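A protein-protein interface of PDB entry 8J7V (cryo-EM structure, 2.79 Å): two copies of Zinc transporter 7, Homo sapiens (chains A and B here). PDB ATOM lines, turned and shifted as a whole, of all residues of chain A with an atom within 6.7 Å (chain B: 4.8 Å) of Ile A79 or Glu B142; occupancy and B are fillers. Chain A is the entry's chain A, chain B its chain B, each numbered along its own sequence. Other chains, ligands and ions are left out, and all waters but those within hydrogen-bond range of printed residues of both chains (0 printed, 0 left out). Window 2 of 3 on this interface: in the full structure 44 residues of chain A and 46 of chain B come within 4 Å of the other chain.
O of Gly A70 sits close to N of Cys A75, 3.4 Å away.
SG of Cys A75 touches CB of Ala B146, 3.7 Å away.
Ile A79 touches Glu B142 (CG2 to CG, 3.5 Å).
Glu B142 touches Ser A80.
OG of Ser B138 touches CB of Phe A83, at 3.2 Å.
Val B141 touches Phe A83.
Of chain B, only Glu B142 comes within 4 Å of Ile A79.
Glu B142 touches just these residues of chain A: Ile A79 (3.5 Å) and Ser A80 (3.4 Å).
Printed residues of chain A within 4 Å of Val B141: Phe A83.
Printed residues of chain B within 4 Å of Cys A75: Ala B146.
Of the printed residues of chain A, Ala B146 touches Cys A75.
Of the printed residues of chain B, Phe A83 touches Ser B138 (3.2 Å) and Val B141 (3.7 Å).
Of the printed residues of chain A, Ser B138 touches Phe A83 (3.2 Å).
Glu A66 touches none of the printed residues of chain B.
Asn A74 touches none of the printed residues of chain B.
The nearest printed residue of chain B that does not touch Ile A79 is Val B141 (5.2 Å).
Hydrophobic or aromatic side chains of chain B that line the printed part of chain A: Val B141 and Ala B146.
Of the 15 printed residues of chain A, 4 touch a printed residue of chain B.
Among the printed residues, no Asp or Glu carboxylate lies within 4 Å of a Lys or Arg side-chain nitrogen of the other chain.
No position is printed for both chains.
Of the 5 pairs that touch across the chains among the printed residues, none has its exchanged pair printed and touching as well.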
ATOM      1  N   GLU A  66       1.457  20.855   4.217  1.00  0.00           N
ATOM      2  CA  GLU A  66       1.401  20.121   5.478  1.00  0.00           C
ATOM      3  C   GLU A  66       1.477  21.059   6.674  1.00  0.00           C
ATOM      4  O   GLU A  66       0.615  21.019   7.557  1.00  0.00           O
ATOM      5  CB  GLU A  66       2.548  19.111   5.531  1.00  0.00           C
ATOM      6  CG  GLU A  66       2.517  18.209   6.734  1.00  0.00           C
ATOM      7  CD  GLU A  66       2.488  16.743   6.383  1.00  0.00           C
ATOM      8  OE1 GLU A  66       2.526  16.423   5.183  1.00  0.00           O
ATOM      9  OE2 GLU A  66       2.416  15.916   7.313  1.00  0.00           O
ATOM     10  N   LEU A  67       2.460  21.958   6.680  1.00  0.00           N
ATOM     11  CA  LEU A  67       2.680  22.826   7.828  1.00  0.00           C
ATOM     12  C   LEU A  67       1.513  23.781   8.018  1.00  0.00           C
ATOM     13  O   LEU A  67       1.207  24.178   9.148  1.00  0.00           O
ATOM     14  CB  LEU A  67       3.991  23.592   7.655  1.00  0.00           C
ATOM     15  CG  LEU A  67       5.177  23.115   8.503  1.00  0.00           C
ATOM     16  CD1 LEU A  67       6.193  24.235   8.729  1.00  0.00           C
ATOM     17  CD2 LEU A  67       4.717  22.510   9.830  1.00  0.00           C
ATOM     18  N   GLY A  70      -1.037  21.871   9.801  1.00  0.00           N
ATOM     19  CA  GLY A  70      -0.587  21.802  11.180  1.00  0.00           C
ATOM     20  C   GLY A  70      -0.883  23.043  11.995  1.00  0.00           C
ATOM     21  O   GLY A  70      -1.441  22.954  13.092  1.00  0.00           O
ATOM     22  N   ASN A  74      -4.275  21.194  13.912  1.00  0.00           N
ATOM     23  CA  ASN A  74      -4.218  19.755  13.707  1.00  0.00           C
ATOM     24  C   ASN A  74      -2.786  19.228  13.719  1.00  0.00           C
ATOM     25  O   ASN A  74      -2.495  18.236  13.044  1.00  0.00           O
ATOM     26  CB  ASN A  74      -4.918  19.389  12.397  1.00  0.00           C
ATOM     27  CG  ASN A  74      -6.158  20.233  12.146  1.00  0.00           C
ATOM     28  OD1 ASN A  74      -7.057  20.301  12.986  1.00  0.00           O
ATOM     29  ND2 ASN A  74      -6.213  20.877  10.986  1.00  0.00           N
ATOM     30  N   CYS A  75      -1.888  19.878  14.465  1.00  0.00           N
ATOM     31  CA  CYS A  75      -0.458  19.612  14.322  1.00  0.00           C
ATOM     32  C   CYS A  75      -0.021  18.362  15.083  1.00  0.00           C
ATOM     33  O   CYS A  75       1.141  17.959  14.984  1.00  0.00           O
ATOM     34  CB  CYS A  75       0.353  20.820  14.790  1.00  0.00           C
ATOM     35  SG  CYS A  75      -0.063  21.391  16.449  1.00  0.00           S
ATOM     36  N   LEU A  76      -0.932  17.742  15.842  1.00  0.00           N
ATOM     37  CA  LEU A  76      -0.639  16.701  16.834  1.00  0.00           C
ATOM     38  C   LEU A  76       0.385  15.643  16.411  1.00  0.00           C
ATOM     39  O   LEU A  76       1.337  15.382  17.154  1.00  0.00           O
ATOM     40  CB  LEU A  76      -1.947  16.014  17.271  1.00  0.00           C
ATOM     41  CG  LEU A  76      -2.927  15.228  16.385  1.00  0.00           C
ATOM     42  CD1 LEU A  76      -3.977  14.561  17.266  1.00  0.00           C
ATOM     43  CD2 LEU A  76      -3.624  16.092  15.344  1.00  0.00           C
ATOM     44  N   GLY A  77       0.216  15.031  15.240  1.00  0.00           N
ATOM     45  CA  GLY A  77       1.237  14.161  14.672  1.00  0.00           C
ATOM     46  C   GLY A  77       1.820  14.805  13.431  1.00  0.00           C
ATOM     47  O   GLY A  77       2.864  14.405  12.889  1.00  0.00           O
ATOM     48  N   LEU A  78       1.106  15.841  12.993  1.00  0.00           N
ATOM     49  CA  LEU A  78       1.427  16.531  11.753  1.00  0.00           C
ATOM     50  C   LEU A  78       2.819  17.150  11.807  1.00  0.00           C
ATOM     51  O   LEU A  78       3.582  17.067  10.844  1.00  0.00           O
ATOM     52  CB  LEU A  78       0.351  17.591  11.498  1.00  0.00           C
ATOM     53  CG  LEU A  78       0.165  18.391  10.206  1.00  0.00           C
ATOM     54  CD1 LEU A  78       1.381  19.227   9.856  1.00  0.00           C
ATOM     55  CD2 LEU A  78      -0.201  17.443   9.061  1.00  0.00           C
ATOM     56  N   ILE A  79       3.157  17.802  12.921  1.00  0.00           N
ATOM     57  CA  ILE A  79       4.421  18.537  13.000  1.00  0.00           C
ATOM     58  C   ILE A  79       5.594  17.563  13.070  1.00  0.00           C
ATOM     59  O   ILE A  79       6.688  17.831  12.558  1.00  0.00           O
ATOM     60  CB  ILE A  79       4.402  19.521  14.185  1.00  0.00           C
ATOM     61  CG1 ILE A  79       5.698  20.338  14.253  1.00  0.00           C
ATOM     62  CG2 ILE A  79       4.123  18.811  15.484  1.00  0.00           C
ATOM     63  CD1 ILE A  79       5.831  21.374  13.161  1.00  0.00           C
ATOM     64  N   SER A  80       5.371  16.399  13.680  1.00  0.00           N
ATOM     65  CA  SER A  80       6.365  15.334  13.671  1.00  0.00           C
ATOM     66  C   SER A  80       6.627  14.847  12.251  1.00  0.00           C
ATOM     67  O   SER A  80       7.787  14.711  11.838  1.00  0.00           O
ATOM     68  CB  SER A  80       5.910  14.168  14.551  1.00  0.00           C
ATOM     69  OG  SER A  80       6.740  13.032  14.371  1.00  0.00           O
ATOM     70  N   ASP A  81       5.549  14.575  11.505  1.00  0.00           N
ATOM     71  CA  ASP A  81       5.680  14.209  10.095  1.00  0.00           C
ATOM     72  C   ASP A  81       6.379  15.316   9.319  1.00  0.00           C
ATOM     73  O   ASP A  81       7.167  15.052   8.404  1.00  0.00           O
ATOM     74  CB  ASP A  81       4.313  13.923   9.469  1.00  0.00           C
ATOM     75  CG  ASP A  81       3.929  12.462   9.548  1.00  0.00           C
ATOM     76  OD1 ASP A  81       4.123  11.852  10.619  1.00  0.00           O
ATOM     77  OD2 ASP A  81       3.448  11.919   8.532  1.00  0.00           O
ATOM     78  N   SER A  82       6.100  16.559   9.707  1.00  0.00           N
ATOM     79  CA  SER A  82       6.668  17.709   9.021  1.00  0.00           C
ATOM     80  C   SER A  82       8.170  17.793   9.231  1.00  0.00           C
ATOM     81  O   SER A  82       8.919  18.139   8.315  1.00  0.00           O
ATOM     82  CB  SER A  82       5.977  18.990   9.489  1.00  0.00           C
ATOM     83  OG  SER A  82       4.581  18.923   9.255  1.00  0.00           O
ATOM     84  N   PHE A  83       8.646  17.479  10.425  1.00  0.00           N
ATOM     85  CA  PHE A  83      10.089  17.583  10.599  1.00  0.00           C
ATOM     86  C   PHE A  83      10.813  16.335  10.095  1.00  0.00           C
ATOM     87  O   PHE A  83      11.953  16.436   9.624  1.00  0.00           O
ATOM     88  CB  PHE A  83      10.426  17.915  12.047  1.00  0.00           C
ATOM     89  CG  PHE A  83      10.242  19.379  12.382  1.00  0.00           C
ATOM     90  CD1 PHE A  83       9.337  20.165  11.684  1.00  0.00           C
ATOM     91  CD2 PHE A  83      10.996  19.975  13.371  1.00  0.00           C
ATOM     92  CE1 PHE A  83       9.175  21.506  11.990  1.00  0.00           C
ATOM     93  CE2 PHE A  83      10.839  21.313  13.684  1.00  0.00           C
ATOM     94  CZ  PHE A  83       9.930  22.080  12.993  1.00  0.00           C
ATOM     95  N   HIS A  84      10.157  15.171  10.117  1.00  0.00           N
ATOM     96  CA  HIS A  84      10.727  14.000   9.449  1.00  0.00           C
ATOM     97  C   HIS A  84      10.889  14.243   7.951  1.00  0.00           C
ATOM     98  O   HIS A  84      11.931  13.930   7.355  1.00  0.00           O
ATOM     99  CB  HIS A  84       9.839  12.783   9.690  1.00  0.00           C
ATOM    100  CG  HIS A  84      10.297  11.927  10.821  1.00  0.00           C
ATOM    101  ND1 HIS A  84      11.629  11.671  11.056  1.00  0.00           N
ATOM    102  CD2 HIS A  84       9.609  11.247  11.766  1.00  0.00           C
ATOM    103  CE1 HIS A  84      11.745  10.883  12.108  1.00  0.00           C
ATOM    104  NE2 HIS A  84      10.534  10.609  12.556  1.00  0.00           N
ATOM    105  N   PHE A  86      11.095  17.238   6.608  1.00  0.00           N
ATOM    106  CA  PHE A  86      12.156  18.219   6.406  1.00  0.00           C
ATOM    107  C   PHE A  86      13.532  17.563   6.433  1.00  0.00           C
ATOM    108  O   PHE A  86      14.441  17.976   5.705  1.00  0.00           O
ATOM    109  CB  PHE A  86      12.058  19.331   7.446  1.00  0.00           C
ATOM    110  CG  PHE A  86      11.072  20.403   7.085  1.00  0.00           C
ATOM    111  CD1 PHE A  86      11.061  20.942   5.809  1.00  0.00           C
ATOM    112  CD2 PHE A  86      10.189  20.897   8.027  1.00  0.00           C
ATOM    113  CE1 PHE A  86      10.165  21.938   5.469  1.00  0.00           C
ATOM    114  CE2 PHE A  86       9.293  21.895   7.694  1.00  0.00           C
ATOM    115  CZ  PHE A  86       9.283  22.416   6.413  1.00  0.00           C
ATOM    116  N   SER B 138      13.878  19.080  16.321  1.00  0.00           N
ATOM    117  CA  SER B 138      12.500  18.679  16.067  1.00  0.00           C
ATOM    118  C   SER B 138      11.688  18.638  17.350  1.00  0.00           C
ATOM    119  O   SER B 138      10.747  19.424  17.531  1.00  0.00           O
ATOM    120  CB  SER B 138      12.480  17.311  15.382  1.00  0.00           C
ATOM    121  OG  SER B 138      12.864  17.411  14.024  1.00  0.00           O
ATOM    122  N   GLU B 139      12.035  17.684  18.221  1.00  0.00           N
ATOM    123  CA  GLU B 139      11.272  17.507  19.483  1.00  0.00           C
ATOM    124  C   GLU B 139      11.071  18.872  20.150  1.00  0.00           C
ATOM    125  O   GLU B 139       9.967  19.106  20.675  1.00  0.00           O
ATOM    126  CB  GLU B 139      11.994  16.528  20.412  1.00  0.00           C
ATOM    127  CG  GLU B 139      11.165  16.132  21.620  1.00  0.00           C
ATOM    128  CD  GLU B 139       9.744  15.705  21.291  1.00  0.00           C
ATOM    129  OE1 GLU B 139       9.583  14.721  20.542  1.00  0.00           O
ATOM    130  OE2 GLU B 139       8.804  16.361  21.781  1.00  0.00           O
ATOM    131  N   GLY B 140      12.088  19.740  20.114  1.00  0.00           N
ATOM    132  CA  GLY B 140      11.902  21.054  20.694  1.00  0.00           C
ATOM    133  C   GLY B 140      10.748  21.802  20.057  1.00  0.00           C
ATOM    134  O   GLY B 140       9.720  22.033  20.705  1.00  0.00           O
ATOM    135  N   VAL B 141      10.889  22.143  18.772  1.00  0.00           N
ATOM    136  CA  VAL B 141       9.944  23.060  18.138  1.00  0.00           C
ATOM    137  C   VAL B 141       8.556  22.439  18.086  1.00  0.00           C
ATOM    138  O   VAL B 141       7.542  23.122  18.285  1.00  0.00           O
ATOM    139  CB  VAL B 141      10.450  23.464  16.741  1.00  0.00           C
ATOM    140  CG1 VAL B 141       9.385  24.233  15.982  1.00  0.00           C
ATOM    141  CG2 VAL B 141      11.709  24.300  16.869  1.00  0.00           C
ATOM    142  N   GLU B 142       8.495  21.130  17.838  1.00  0.00           N
ATOM    143  CA  GLU B 142       7.265  20.362  17.969  1.00  0.00           C
ATOM    144  C   GLU B 142       6.587  20.619  19.311  1.00  0.00           C
ATOM    145  O   GLU B 142       5.442  21.087  19.366  1.00  0.00           O
ATOM    146  CB  GLU B 142       7.590  18.876  17.785  1.00  0.00           C
ATOM    147  CG  GLU B 142       6.419  17.933  17.938  1.00  0.00           C
ATOM    148  CD  GLU B 142       6.779  16.516  17.546  1.00  0.00           C
ATOM    149  OE1 GLU B 142       7.941  16.293  17.147  1.00  0.00           O
ATOM    150  OE2 GLU B 142       5.905  15.627  17.631  1.00  0.00           O
ATOM    151  N   ARG B 143       7.313  20.328  20.393  1.00  0.00           N
ATOM    152  CA  ARG B 143       6.774  20.618  21.746  1.00  0.00           C
ATOM    153  C   ARG B 143       6.448  22.111  21.818  1.00  0.00           C
ATOM    154  O   ARG B 143       5.423  22.461  22.437  1.00  0.00           O
ATOM    155  CB  ARG B 143       7.797  20.224  22.815  1.00  0.00           C
ATOM    156  CG  ARG B 143       7.376  20.548  24.241  1.00  0.00           C
ATOM    157  CD  ARG B 143       6.152  19.765  24.679  1.00  0.00           C
ATOM    158  NE  ARG B 143       5.816  20.020  26.072  1.00  0.00           N
ATOM    159  CZ  ARG B 143       4.797  19.462  26.715  1.00  0.00           C
ATOM    160  NH1 ARG B 143       3.980  18.644  26.075  1.00  0.00           N
ATOM    161  NH2 ARG B 143       4.599  19.725  27.995  1.00  0.00           N
ATOM    162  N   ALA B 144       7.276  22.956  21.191  1.00  0.00           N
ATOM    163  CA  ALA B 144       7.048  24.394  21.294  1.00  0.00           C
ATOM    164  C   ALA B 144       5.664  24.781  20.789  1.00  0.00           C
ATOM    165  O   ALA B 144       5.152  25.848  21.143  1.00  0.00           O
ATOM    166  CB  ALA B 144       8.123  25.156  20.524  1.00  0.00           C
ATOM    167  N   LEU B 145       5.044  23.938  19.961  1.00  0.00           N
ATOM    168  CA  LEU B 145       3.736  24.289  19.421  1.00  0.00           C
ATOM    169  C   LEU B 145       2.607  23.649  20.220  1.00  0.00           C
ATOM    170  O   LEU B 145       1.748  24.354  20.760  1.00  0.00           O
ATOM    171  CB  LEU B 145       3.655  23.884  17.947  1.00  0.00           C
ATOM    172  CG  LEU B 145       3.816  25.010  16.920  1.00  0.00           C
ATOM    173  CD1 LEU B 145       2.540  25.828  16.804  1.00  0.00           C
ATOM    174  CD2 LEU B 145       5.002  25.906  17.267  1.00  0.00           C
ATOM    175  N   ALA B 146       2.591  22.324  20.309  1.00  0.00           N
ATOM    176  CA  ALA B 146       1.545  21.628  21.044  1.00  0.00           C
ATOM    177  C   ALA B 146       2.112  20.420  21.787  1.00  0.00           C
ATOM    178  O   ALA B 146       2.946  19.689  21.256  1.00  0.00           O
ATOM    179  CB  ALA B 146       0.419  21.204  20.096  1.00  0.00           C
